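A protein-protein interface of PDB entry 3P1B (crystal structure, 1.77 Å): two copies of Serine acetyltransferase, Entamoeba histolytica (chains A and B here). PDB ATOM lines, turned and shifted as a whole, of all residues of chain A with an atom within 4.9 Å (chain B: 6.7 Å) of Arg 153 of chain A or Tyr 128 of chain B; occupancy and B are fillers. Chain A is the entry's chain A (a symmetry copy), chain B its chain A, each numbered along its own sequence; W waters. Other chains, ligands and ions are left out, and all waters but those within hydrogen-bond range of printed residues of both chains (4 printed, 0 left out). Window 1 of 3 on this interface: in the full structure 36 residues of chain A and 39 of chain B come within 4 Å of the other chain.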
ATOM      1  N   ARG A 149      22.573  38.547  -9.070  1.00  0.00           N
ATOM      2  CA  ARG A 149      23.550  37.510  -8.876  1.00  0.00           C
ATOM      3  C   ARG A 149      22.987  36.090  -8.731  1.00  0.00           C
ATOM      4  O   ARG A 149      23.708  35.154  -8.637  1.00  0.00           O
ATOM      5  CB  ARG A 149      24.510  37.895  -7.739  1.00  0.00           C
ATOM      6  CG  ARG A 149      25.305  39.170  -7.932  1.00  0.00           C
ATOM      7  CD  ARG A 149      26.636  38.890  -8.553  1.00  0.00           C
ATOM      8  NE  ARG A 149      27.462  40.021  -8.836  1.00  0.00           N
ATOM      9  CZ  ARG A 149      27.214  40.951  -9.738  1.00  0.00           C
ATOM     10  NH1 ARG A 149      26.101  40.939 -10.417  1.00  0.00           N
ATOM     11  NH2 ARG A 149      28.096  41.909  -9.942  1.00  0.00           N
ATOM     12  N   TYR A 150      21.678  35.985  -8.744  1.00  0.00           N
ATOM     13  CA  TYR A 150      21.016  34.741  -8.589  1.00  0.00           C
ATOM     14  C   TYR A 150      20.273  34.273  -9.842  1.00  0.00           C
ATOM     15  O   TYR A 150      20.628  33.277 -10.438  1.00  0.00           O
ATOM     16  CB  TYR A 150      20.075  34.825  -7.386  1.00  0.00           C
ATOM     17  CG  TYR A 150      20.836  34.842  -6.058  1.00  0.00           C
ATOM     18  CD1 TYR A 150      20.911  33.731  -5.297  1.00  0.00           C
ATOM     19  CD2 TYR A 150      21.466  35.962  -5.608  1.00  0.00           C
ATOM     20  CE1 TYR A 150      21.588  33.700  -4.148  1.00  0.00           C
ATOM     21  CE2 TYR A 150      22.124  35.955  -4.443  1.00  0.00           C
ATOM     22  CZ  TYR A 150      22.190  34.807  -3.710  1.00  0.00           C
ATOM     23  OH  TYR A 150      22.860  34.789  -2.556  1.00  0.00           O
ATOM     24  N   TYR A 151      19.221  34.975 -10.181  1.00  0.00           N
ATOM     25  CA  TYR A 151      18.430  34.519 -11.306  1.00  0.00           C
ATOM     26  C   TYR A 151      19.258  34.433 -12.587  1.00  0.00           C
ATOM     27  O   TYR A 151      18.971  33.558 -13.413  1.00  0.00           O
ATOM     28  CB  TYR A 151      17.134  35.289 -11.483  1.00  0.00           C
ATOM     29  CG  TYR A 151      16.428  34.989 -12.778  1.00  0.00           C
ATOM     30  CD1 TYR A 151      15.973  33.681 -13.078  1.00  0.00           C
ATOM     31  CD2 TYR A 151      16.184  36.011 -13.700  1.00  0.00           C
ATOM     32  CE1 TYR A 151      15.354  33.397 -14.263  1.00  0.00           C
ATOM     33  CE2 TYR A 151      15.497  35.747 -14.875  1.00  0.00           C
ATOM     34  CZ  TYR A 151      15.090  34.450 -15.148  1.00  0.00           C
ATOM     35  OH  TYR A 151      14.428  34.187 -16.331  1.00  0.00           O
ATOM     36  N   CYS A 152      20.277  35.298 -12.720  1.00  0.00           N
ATOM     37  CA  CYS A 152      21.052  35.342 -13.942  1.00  0.00           C
ATOM     38  C   CYS A 152      21.958  34.101 -14.029  1.00  0.00           C
ATOM     39  O   CYS A 152      22.182  33.563 -15.106  1.00  0.00           O
ATOM     40  CB  CYS A 152      21.857  36.646 -14.052  1.00  0.00           C
ATOM     41  SG  CYS A 152      23.133  36.866 -12.853  1.00  0.00           S
ATOM     42  N   ARG A 153      22.421  33.611 -12.880  1.00  0.00           N
ATOM     43  CA  ARG A 153      23.140  32.327 -12.867  1.00  0.00           C
ATOM     44  C   ARG A 153      22.182  31.164 -13.191  1.00  0.00           C
ATOM     45  O   ARG A 153      22.595  30.237 -13.863  1.00  0.00           O
ATOM     46  CB  ARG A 153      23.794  32.101 -11.523  1.00  0.00           C
ATOM     47  CG  ARG A 153      24.548  30.797 -11.473  1.00  0.00           C
ATOM     48  CD  ARG A 153      25.922  30.881 -12.226  1.00  0.00           C
ATOM     49  NE  ARG A 153      26.481  29.528 -12.318  1.00  0.00           N
ATOM     50  CZ  ARG A 153      27.329  29.051 -11.418  1.00  0.00           C
ATOM     51  NH1 ARG A 153      27.698  29.849 -10.414  1.00  0.00           N
ATOM     52  NH2 ARG A 153      27.799  27.812 -11.512  1.00  0.00           N
ATOM     53  N   GLU A 154      20.909  31.254 -12.784  1.00  0.00           N
ATOM     54  CA  GLU A 154      19.925  30.178 -12.964  1.00  0.00           C
ATOM     55  C   GLU A 154      19.484  30.064 -14.432  1.00  0.00           C
ATOM     56  O   GLU A 154      19.346  28.941 -14.956  1.00  0.00           O
ATOM     57  CB  GLU A 154      18.665  30.387 -12.091  1.00  0.00           C
ATOM     58  CG  GLU A 154      17.488  29.376 -12.248  1.00  0.00           C
ATOM     59  CD  GLU A 154      16.372  29.598 -11.204  1.00  0.00           C
ATOM     60  OE1 GLU A 154      15.429  30.376 -11.448  1.00  0.00           O
ATOM     61  OE2 GLU A 154      16.408  28.993 -10.132  1.00  0.00           O
ATOM     62  N   MET A 155      19.309  31.223 -15.088  1.00  0.00           N
ATOM     63  CA  MET A 155      19.214  31.237 -16.581  1.00  0.00           C
ATOM     64  C   MET A 155      20.281  30.438 -17.319  1.00  0.00           C
ATOM     65  O   MET A 155      19.934  29.624 -18.188  1.00  0.00           O
ATOM     66  CB  MET A 155      19.246  32.673 -17.164  1.00  0.00           C
ATOM     67  CG  MET A 155      18.204  33.577 -16.598  1.00  0.00           C
ATOM     68  SD  MET A 155      18.024  35.177 -17.480  1.00  0.00           S
ATOM     69  CE  MET A 155      18.349  34.605 -19.081  1.00  0.00           C
ATOM     70  N   MET A 156      21.551  30.695 -17.026  1.00  0.00           N
ATOM     71  CA  MET A 156      22.678  30.082 -17.671  1.00  0.00           C
ATOM     72  C   MET A 156      22.766  28.593 -17.266  1.00  0.00           C
ATOM     73  O   MET A 156      23.297  27.783 -18.004  1.00  0.00           O
ATOM     74  CB  MET A 156      23.963  30.848 -17.348  1.00  0.00           C
ATOM     75  CG  MET A 156      23.885  32.335 -17.863  1.00  0.00           C
ATOM     76  SD  MET A 156      23.270  32.454 -19.550  1.00  0.00           S
ATOM     77  CE  MET A 156      24.652  31.585 -20.280  1.00  0.00           C
ATOM     78  N   GLU A 157      22.255  28.267 -16.079  1.00  0.00           N
ATOM     79  CA  GLU A 157      22.118  26.859 -15.716  1.00  0.00           C
ATOM     80  C   GLU A 157      21.059  26.118 -16.597  1.00  0.00           C
ATOM     81  O   GLU A 157      21.163  24.902 -16.845  1.00  0.00           O
ATOM     82  CB  GLU A 157      21.937  26.663 -14.192  1.00  0.00           C
ATOM     83  CG  GLU A 157      23.173  26.944 -13.366  1.00  0.00           C
ATOM     84  CD  GLU A 157      24.415  26.157 -13.787  1.00  0.00           C
ATOM     85  OE1 GLU A 157      24.287  25.074 -14.401  1.00  0.00           O
ATOM     86  OE2 GLU A 157      25.532  26.621 -13.487  1.00  0.00           O
ATOM     87  N   HIS A 168      29.335  31.782 -17.405  1.00  0.00           N
ATOM     88  CA  HIS A 168      28.903  32.551 -16.293  1.00  0.00           C
ATOM     89  C   HIS A 168      28.434  33.885 -16.829  1.00  0.00           C
ATOM     90  O   HIS A 168      29.139  34.489 -17.662  1.00  0.00           O
ATOM     91  CB  HIS A 168      30.086  32.846 -15.435  1.00  0.00           C
ATOM     92  CG  HIS A 168      29.684  33.364 -14.106  1.00  0.00           C
ATOM     93  ND1 HIS A 168      29.757  32.603 -12.958  1.00  0.00           N
ATOM     94  CD2 HIS A 168      29.120  34.543 -13.746  1.00  0.00           C
ATOM     95  CE1 HIS A 168      29.304  33.314 -11.941  1.00  0.00           C
ATOM     96  NE2 HIS A 168      28.891  34.480 -12.396  1.00  0.00           N
ATOM     97  N   PRO A 169      27.278  34.345 -16.378  1.00  0.00           N
ATOM     98  CA  PRO A 169      26.763  35.589 -16.882  1.00  0.00           C
ATOM     99  C   PRO A 169      27.585  36.878 -16.691  1.00  0.00           C
ATOM    100  O   PRO A 169      27.247  37.891 -17.359  1.00  0.00           O
ATOM    101  CB  PRO A 169      25.393  35.717 -16.204  1.00  0.00           C
ATOM    102  CG  PRO A 169      25.496  34.897 -14.939  1.00  0.00           C
ATOM    103  CD  PRO A 169      26.417  33.753 -15.331  1.00  0.00           C
ATOM    104  N   ARG B  43      15.192  16.750  -3.687  1.00  0.00           N
ATOM    105  CA  ARG B  43      15.241  18.196  -3.424  1.00  0.00           C
ATOM    106  C   ARG B  43      14.241  18.719  -2.368  1.00  0.00           C
ATOM    107  O   ARG B  43      14.661  19.376  -1.416  1.00  0.00           O
ATOM    108  CB  ARG B  43      14.903  19.001  -4.683  1.00  0.00           C
ATOM    109  CG  ARG B  43      15.882  19.045  -5.752  1.00  0.00           C
ATOM    110  CD  ARG B  43      15.112  19.634  -6.902  1.00  0.00           C
ATOM    111  NE  ARG B  43      16.064  20.296  -7.706  1.00  0.00           N
ATOM    112  CZ  ARG B  43      15.853  21.088  -8.745  1.00  0.00           C
ATOM    113  NH1 ARG B  43      14.656  21.486  -9.123  1.00  0.00           N
ATOM    114  NH2 ARG B  43      16.936  21.556  -9.340  1.00  0.00           N
ATOM    115  N   ALA B 111      31.004  23.022  -1.518  1.00  0.00           N
ATOM    116  CA  ALA B 111      30.711  23.811  -2.732  1.00  0.00           C
ATOM    117  C   ALA B 111      30.892  25.357  -2.517  1.00  0.00           C
ATOM    118  O   ALA B 111      31.567  26.004  -3.307  1.00  0.00           O
ATOM    119  CB  ALA B 111      29.314  23.523  -3.247  1.00  0.00           C
ATOM    120  N   TYR B 112      30.238  25.915  -1.504  1.00  0.00           N
ATOM    121  CA  TYR B 112      30.457  27.318  -1.152  1.00  0.00           C
ATOM    122  C   TYR B 112      31.956  27.623  -0.926  1.00  0.00           C
ATOM    123  O   TYR B 112      32.495  28.617  -1.460  1.00  0.00           O
ATOM    124  CB  TYR B 112      29.595  27.714   0.052  1.00  0.00           C
ATOM    125  CG  TYR B 112      29.662  29.200   0.255  1.00  0.00           C
ATOM    126  CD1 TYR B 112      28.833  30.057  -0.482  1.00  0.00           C
ATOM    127  CD2 TYR B 112      30.624  29.753   1.103  1.00  0.00           C
ATOM    128  CE1 TYR B 112      28.921  31.454  -0.334  1.00  0.00           C
ATOM    129  CE2 TYR B 112      30.712  31.159   1.269  1.00  0.00           C
ATOM    130  CZ  TYR B 112      29.860  31.978   0.552  1.00  0.00           C
ATOM    131  OH  TYR B 112      29.957  33.333   0.736  1.00  0.00           O
ATOM    132  N   ASP B 115      34.169  27.660  -4.298  1.00  0.00           N
ATOM    133  CA  ASP B 115      33.684  28.358  -5.496  1.00  0.00           C
ATOM    134  C   ASP B 115      33.555  29.868  -5.255  1.00  0.00           C
ATOM    135  O   ASP B 115      32.541  30.369  -4.700  1.00  0.00           O
ATOM    136  CB  ASP B 115      32.350  27.759  -5.941  1.00  0.00           C
ATOM    137  CG  ASP B 115      31.798  28.415  -7.220  1.00  0.00           C
ATOM    138  OD1 ASP B 115      32.479  29.273  -7.803  1.00  0.00           O
ATOM    139  OD2 ASP B 115      30.608  28.131  -7.579  1.00  0.00           O
ATOM    140  N   ALA B 117      32.839  32.032  -7.217  1.00  0.00           N
ATOM    141  CA  ALA B 117      31.591  32.497  -7.818  1.00  0.00           C
ATOM    142  C   ALA B 117      30.265  32.260  -7.056  1.00  0.00           C
ATOM    143  O   ALA B 117      29.231  32.881  -7.396  1.00  0.00           O
ATOM    144  CB  ALA B 117      31.475  32.037  -9.293  1.00  0.00           C
ATOM    145  N   ALA B 118      30.234  31.423  -6.007  1.00  0.00           N
ATOM    146  CA  ALA B 118      28.955  31.228  -5.301  1.00  0.00           C
ATOM    147  C   ALA B 118      28.585  32.379  -4.320  1.00  0.00           C
ATOM    148  O   ALA B 118      29.407  32.697  -3.429  1.00  0.00           O
ATOM    149  CB  ALA B 118      28.946  29.838  -4.549  1.00  0.00           C
ATOM    150  N   PRO B 119      27.362  32.963  -4.470  1.00  0.00           N
ATOM    151  CA  PRO B 119      26.715  34.037  -3.700  1.00  0.00           C
ATOM    152  C   PRO B 119      26.137  33.580  -2.351  1.00  0.00           C
ATOM    153  O   PRO B 119      26.173  34.330  -1.362  1.00  0.00           O
ATOM    154  CB  PRO B 119      25.568  34.503  -4.640  1.00  0.00           C
ATOM    155  CG  PRO B 119      25.266  33.359  -5.454  1.00  0.00           C
ATOM    156  CD  PRO B 119      26.631  32.722  -5.725  1.00  0.00           C
ATOM    157  N   GLY B 120      25.660  32.351  -2.294  1.00  0.00           N
ATOM    158  CA  GLY B 120      25.067  31.771  -1.083  1.00  0.00           C
ATOM    159  C   GLY B 120      24.663  30.337  -1.388  1.00  0.00           C
ATOM    160  O   GLY B 120      24.675  29.894  -2.548  1.00  0.00           O
ATOM    161  N   LEU B 123      21.616  29.312  -3.967  1.00  0.00           N
ATOM    162  CA  LEU B 123      21.954  29.125  -5.402  1.00  0.00           C
ATOM    163  C   LEU B 123      22.484  27.735  -5.786  1.00  0.00           C
ATOM    164  O   LEU B 123      22.061  27.151  -6.816  1.00  0.00           O
ATOM    165  CB  LEU B 123      22.903  30.239  -5.895  1.00  0.00           C
ATOM    166  CG  LEU B 123      23.047  30.244  -7.417  1.00  0.00           C
ATOM    167  CD1 LEU B 123      21.732  30.625  -8.085  1.00  0.00           C
ATOM    168  CD2 LEU B 123      24.132  31.196  -7.911  1.00  0.00           C
ATOM    169  N   ILE B 124      23.443  27.243  -4.984  1.00  0.00           N
ATOM    170  CA  ILE B 124      23.937  25.874  -5.051  1.00  0.00           C
ATOM    171  C   ILE B 124      22.803  24.869  -4.960  1.00  0.00           C
ATOM    172  O   ILE B 124      22.590  24.007  -5.855  1.00  0.00           O
ATOM    173  CB  ILE B 124      25.038  25.624  -4.010  1.00  0.00           C
ATOM    174  CG1 ILE B 124      25.945  26.887  -3.980  1.00  0.00           C
ATOM    175  CG2 ILE B 124      25.773  24.209  -4.295  1.00  0.00           C
ATOM    176  CD1 ILE B 124      27.132  26.834  -3.037  1.00  0.00           C
ATOM    177  N   ILE B 125      22.027  25.004  -3.900  1.00  0.00           N
ATOM    178  CA  ILE B 125      20.945  24.113  -3.637  1.00  0.00           C
ATOM    179  C   ILE B 125      19.978  24.104  -4.841  1.00  0.00           C
ATOM    180  O   ILE B 125      19.623  23.050  -5.306  1.00  0.00           O
ATOM    181  CB  ILE B 125      20.202  24.542  -2.356  1.00  0.00           C
ATOM    182  CG1 ILE B 125      21.071  24.291  -1.109  1.00  0.00           C
ATOM    183  CG2 ILE B 125      18.845  23.847  -2.242  1.00  0.00           C
ATOM    184  CD1 ILE B 125      20.427  24.751   0.201  1.00  0.00           C
ATOM    185  N   ARG B 126      19.642  25.266  -5.364  1.00  0.00           N
ATOM    186  CA  ARG B 126      18.675  25.391  -6.433  1.00  0.00           C
ATOM    187  C   ARG B 126      19.127  24.943  -7.817  1.00  0.00           C
ATOM    188  O   ARG B 126      18.364  24.392  -8.525  1.00  0.00           O
ATOM    189  CB  ARG B 126      18.202  26.820  -6.599  1.00  0.00           C
ATOM    190  CG  ARG B 126      17.617  27.478  -5.419  1.00  0.00           C
ATOM    191  CD  ARG B 126      16.202  27.534  -5.531  1.00  0.00           C
ATOM    192  NE  ARG B 126      15.800  27.990  -6.821  1.00  0.00           N
ATOM    193  CZ  ARG B 126      14.646  27.679  -7.350  1.00  0.00           C
ATOM    194  NH1 ARG B 126      13.793  26.881  -6.706  1.00  0.00           N
ATOM    195  NH2 ARG B 126      14.345  28.120  -8.521  1.00  0.00           N
ATOM    196  N   CYS B 127      20.366  25.214  -8.186  1.00  0.00           N
ATOM    197  CA  CYS B 127      20.706  25.165  -9.580  1.00  0.00           C
ATOM    198  C   CYS B 127      22.096  24.638  -9.889  1.00  0.00           C
ATOM    199  O   CYS B 127      22.417  24.456 -11.018  1.00  0.00           O
ATOM    200  CB  CYS B 127      20.419  26.537 -10.228  1.00  0.00           C
ATOM    201  SG  CYS B 127      21.638  27.654 -10.035  1.00  0.00           S
ATOM    202  N   TYR B 128      22.904  24.368  -8.877  1.00  0.00           N
ATOM    203  CA  TYR B 128      24.255  23.896  -9.148  1.00  0.00           C
ATOM    204  C   TYR B 128      24.273  22.395  -9.590  1.00  0.00           C
ATOM    205  O   TYR B 128      23.838  21.567  -8.834  1.00  0.00           O
ATOM    206  CB  TYR B 128      25.172  24.086  -7.968  1.00  0.00           C
ATOM    207  CG  TYR B 128      25.953  25.375  -7.930  1.00  0.00           C
ATOM    208  CD1 TYR B 128      27.296  25.395  -7.539  1.00  0.00           C
ATOM    209  CD2 TYR B 128      25.365  26.553  -8.263  1.00  0.00           C
ATOM    210  CE1 TYR B 128      28.010  26.561  -7.485  1.00  0.00           C
ATOM    211  CE2 TYR B 128      26.061  27.709  -8.190  1.00  0.00           C
ATOM    212  CZ  TYR B 128      27.377  27.721  -7.819  1.00  0.00           C
ATOM    213  OH  TYR B 128      28.048  28.862  -7.758  1.00  0.00           O
ATOM    214  N   PRO B 129      24.822  22.079 -10.768  1.00  0.00           N
ATOM    215  CA  PRO B 129      24.618  20.729 -11.322  1.00  0.00           C
ATOM    216  C   PRO B 129      25.365  19.668 -10.553  1.00  0.00           C
ATOM    217  O   PRO B 129      24.820  18.561 -10.419  1.00  0.00           O
ATOM    218  CB  PRO B 129      25.133  20.834 -12.790  1.00  0.00           C
ATOM    219  CG  PRO B 129      26.210  21.966 -12.691  1.00  0.00           C
ATOM    220  CD  PRO B 129      25.689  22.927 -11.616  1.00  0.00           C
ATOM    221  N   GLY B 130      26.645  19.973 -10.202  1.00  0.00           N
ATOM    222  CA  GLY B 130      27.387  19.165  -9.190  1.00  0.00           C
ATOM    223  C   GLY B 130      26.502  18.699  -8.024  1.00  0.00           C
ATOM    224  O   GLY B 130      26.448  17.493  -7.662  1.00  0.00           O
ATOM    225  N   PHE B 131      25.739  19.624  -7.478  1.00  0.00           N
ATOM    226  CA  PHE B 131      24.942  19.296  -6.351  1.00  0.00           C
ATOM    227  C   PHE B 131      23.712  18.465  -6.662  1.00  0.00           C
ATOM    228  O   PHE B 131      23.375  17.549  -5.895  1.00  0.00           O
ATOM    229  CB  PHE B 131      24.570  20.533  -5.553  1.00  0.00           C
ATOM    230  CG  PHE B 131      24.015  20.210  -4.195  1.00  0.00           C
ATOM    231  CD1 PHE B 131      24.815  19.592  -3.228  1.00  0.00           C
ATOM    232  CD2 PHE B 131      22.696  20.409  -3.929  1.00  0.00           C
ATOM    233  CE1 PHE B 131      24.356  19.272  -2.004  1.00  0.00           C
ATOM    234  CE2 PHE B 131      22.178  20.087  -2.605  1.00  0.00           C
ATOM    235  CZ  PHE B 131      23.017  19.495  -1.665  1.00  0.00           C
ATOM    236  N   GLN B 132      23.059  18.724  -7.790  1.00  0.00           N
ATOM    237  CA  GLN B 132      21.906  17.897  -8.182  1.00  0.00           C
ATOM    238  C   GLN B 132      22.456  16.461  -8.393  1.00  0.00           C
ATOM    239  O   GLN B 132      21.881  15.523  -7.828  1.00  0.00           O
ATOM    240  CB  GLN B 132      21.190  18.454  -9.405  1.00  0.00           C
ATOM    241  CG  GLN B 132      21.065  20.005  -9.390  1.00  0.00           C
ATOM    242  CD  GLN B 132      20.394  20.545  -8.102  1.00  0.00           C
ATOM    243  OE1 GLN B 132      19.311  20.112  -7.757  1.00  0.00           O
ATOM    244  NE2 GLN B 132      21.049  21.498  -7.417  1.00  0.00           N
ATOM    245  N   ALA B 133      23.588  16.310  -9.077  1.00  0.00           N
ATOM    246  CA  ALA B 133      24.199  14.981  -9.308  1.00  0.00           C
ATOM    247  C   ALA B 133      24.383  14.188  -8.018  1.00  0.00           C
ATOM    248  O   ALA B 133      24.133  12.975  -7.988  1.00  0.00           O
ATOM    249  CB  ALA B 133      25.508  15.032 -10.108  1.00  0.00           C
ATOM    250  N   THR B 163      22.850  16.799 -16.552  1.00  0.00           N
ATOM    251  CA  THR B 163      23.958  17.592 -16.092  1.00  0.00           C
ATOM    252  C   THR B 163      25.227  17.290 -16.840  1.00  0.00           C
ATOM    253  O   THR B 163      26.242  17.962 -16.622  1.00  0.00           O
ATOM    254  CB  THR B 163      24.280  17.318 -14.579  1.00  0.00           C
ATOM    255  OG1 THR B 163      24.601  15.943 -14.397  1.00  0.00           O
ATOM    256  CG2 THR B 163      23.050  17.654 -13.721  1.00  0.00           C
ATOM    257  N   PHE B 178      32.689  18.111  -3.837  1.00  0.00           N
ATOM    258  CA  PHE B 178      32.289  19.185  -4.787  1.00  0.00           C
ATOM    259  C   PHE B 178      32.822  18.989  -6.220  1.00  0.00           C
ATOM    260  O   PHE B 178      34.023  18.916  -6.464  1.00  0.00           O
ATOM    261  CB  PHE B 178      32.605  20.597  -4.189  1.00  0.00           C
ATOM    262  CG  PHE B 178      32.410  21.787  -5.129  1.00  0.00           C
ATOM    263  CD1 PHE B 178      31.216  22.020  -5.800  1.00  0.00           C
ATOM    264  CD2 PHE B 178      33.451  22.704  -5.298  1.00  0.00           C
ATOM    265  CE1 PHE B 178      31.064  23.156  -6.648  1.00  0.00           C
ATOM    266  CE2 PHE B 178      33.299  23.848  -6.154  1.00  0.00           C
ATOM    267  CZ  PHE B 178      32.099  24.069  -6.779  1.00  0.00           C
ATOM    268  N   ILE B 179      31.896  18.893  -7.159  1.00  0.00           N
ATOM    269  CA  ILE B 179      32.202  18.863  -8.614  1.00  0.00           C
ATOM    270  C   ILE B 179      31.878  20.273  -9.142  1.00  0.00           C
ATOM    271  O   ILE B 179      30.748  20.672  -9.153  1.00  0.00           O
ATOM    272  CB  ILE B 179      31.294  17.814  -9.325  1.00  0.00           C
ATOM    273  CG1 ILE B 179      31.732  16.341  -9.018  1.00  0.00           C
ATOM    274  CG2 ILE B 179      31.155  18.087 -10.778  1.00  0.00           C
ATOM    275  CD1 ILE B 179      30.472  15.468  -9.098  1.00  0.00           C
ATOM    276  N   ASP B 180      32.862  21.047  -9.590  1.00  0.00           N
ATOM    277  CA  ASP B 180      32.513  22.387 -10.112  1.00  0.00           C
ATOM    278  C   ASP B 180      32.368  22.370 -11.620  1.00  0.00           C
ATOM    279  O   ASP B 180      33.233  21.887 -12.309  1.00  0.00           O
ATOM    280  CB  ASP B 180      33.595  23.371  -9.701  1.00  0.00           C
ATOM    281  CG  ASP B 180      33.152  24.852  -9.798  1.00  0.00           C
ATOM    282  OD1 ASP B 180      31.949  25.221 -10.050  1.00  0.00           O
ATOM    283  OD2 ASP B 180      34.018  25.704  -9.505  1.00  0.00           O
ATOM    284  N   HIS B 181      31.257  22.919 -12.117  1.00  0.00           N
ATOM    285  CA  HIS B 181      30.913  22.964 -13.558  1.00  0.00           C
ATOM    286  C   HIS B 181      30.408  21.603 -14.086  1.00  0.00           C
ATOM    287  O   HIS B 181      29.206  21.446 -14.416  1.00  0.00           O
ATOM    288  CB  HIS B 181      32.062  23.566 -14.390  1.00  0.00           C
ATOM    289  CG  HIS B 181      32.499  24.914 -13.906  1.00  0.00           C
ATOM    290  ND1 HIS B 181      33.719  25.135 -13.314  1.00  0.00           N
ATOM    291  CD2 HIS B 181      31.820  26.086 -13.815  1.00  0.00           C
ATOM    292  CE1 HIS B 181      33.808  26.404 -12.948  1.00  0.00           C
ATOM    293  NE2 HIS B 181      32.667  26.997 -13.232  1.00  0.00           N
HETATM  294  O   HOH W   1      30.761  27.454 -10.258  1.00  0.00           O
HETATM  295  O   HOH W   2      28.840  24.553 -10.845  1.00  0.00           O
HETATM  296  O   HOH W   3      31.064  29.601 -12.306  1.00  0.00           O
HETATM  297  O   HOH W   4      27.267  32.374  -9.565  1.00  0.00           O
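NH2 of Arg 126 of chain B is in salt-bridge range of OE2 of Glu 154 of chain A.
OH of Tyr 128 of chain B lies within hydrogen-bond range of NH1 of Arg 153 of chain A, at 2.9 Å.
The guanidinium group (NH2) of Arg 43 of chain B is in hydrogen-bond range of the backbone carbonyl oxygen (O) of Arg 126 of chain B (3.3 Å).
The side-chain carboxylate of Asp 115 of chain B lies within hydrogen-bond range of the backbone NH of Ala 117 of chain B, at 2.8 Å.
OH of Tyr 128 of chain B lies within hydrogen-bond range of OD2 of Asp 115 of chain B, at 2.7 Å.
The backbone carbonyl oxygen (O) of Leu 123 of chain B sits at hydrogen-bond distance from the side-chain sulfur (SG) of Cys 127 of chain B.
The backbone carbonyl oxygen of Tyr 128 of chain B lies within hydrogen-bond range of the side-chain amide nitrogen of Gln 132 of chain B, at 3.1 Å.
The guanidinium group (NH2) of Arg 153 of chain A lies within salt-bridge range of the side-chain carboxylate (OE2) of Glu 157 of chain A, 3.2 Å away.
Among the printed residues, pairs that only touch across the chains: Arg 149 of chain A with Pro 119 of chain B, Tyr 150 of chain A with Pro 119 of chain B, Tyr 150 of chain A with Gly 120 of chain B, Tyr 150 of chain A with Leu 123 of chain B, Arg 153 of chain A with Leu 123 of chain B, Glu 157 of chain A with Cys 127 of chain B, Glu 157 of chain A with Pro 129 of chain B and His 168 of chain A with Ala 117 of chain B.
Of chain B, only Leu 123 and Tyr 128 come within 4 Å of Arg 153 of chain A.
Tyr 128 of chain B touches one residue of chain A.
Of the printed residues of chain A, Pro 119 of chain B touches Arg 149 (3.97 Å) and Tyr 150 (3.4 Å).
Of the printed residues of chain B, Glu 154 of chain A touches Arg 126 (2.8 Å).
Of the printed residues of chain B, His 168 of chain A touches Ala 117.
His 181 of chain B touches none of the printed residues of chain A.
Asp 180 of chain B touches none of the printed residues of chain A.
The nearest residue of chain B that does not touch Arg 153 of chain A is Asp 115 of chain B (4.4 Å).
The nearest printed residue of chain A that does not touch Pro 129 of chain B is Arg 153 of chain A (5.3 Å).
Of the 24 printed residues of chain B, 8 touch a printed residue of chain A.
Hydrophobic or aromatic side chains of chain B within 4 Å of the printed part of chain A: Ala 117, Pro 119, Leu 123, Tyr 128 and Pro 129.
Of the 11 printed residues of chain A, 6 touch a printed residue of chain B.
Hydrophobic or aromatic side chains of chain A within 4 Å of the printed part of chain B: Tyr 150 and His 168.
Among the printed residues, 10 pairs touch across the chains.
Among the printed residues, Asp or Glu carboxylates within 4 Å of a Lys or Arg side-chain nitrogen of the other chain: Glu 154 of chain A with Arg 126 of chain B.
No position is printed for both chains.
Of the 10 pairs that touch across the chains among the printed residues, none has its exchanged pair printed and touching as well.
Water W1 lies within hydrogen-bond range of OD1 of Asp 180 of chain B (2.5 Å), OD2 of Asp 115 of chain B (2.8 Å) and NH2 of Arg 153 of chain A (3.2 Å).
Water W4 bridges the guanidinium group (NH1) of Arg 153 of chain A (2.7 Å) and the backbone carbonyl oxygen (O) of Ala 117 of chain B (3.0 Å).
Water W2 lies within hydrogen-bond range of N of His 181 of chain B (3.2 Å), OD1 of Asp 180 of chain B (3.3 Å) and NH2 of Arg 153 of chain A (3.5 Å).
Water W3 bridges NE2 of His 181 of chain B (3.2 Å) and ND1 of His 168 of chain A (3.3 Å).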
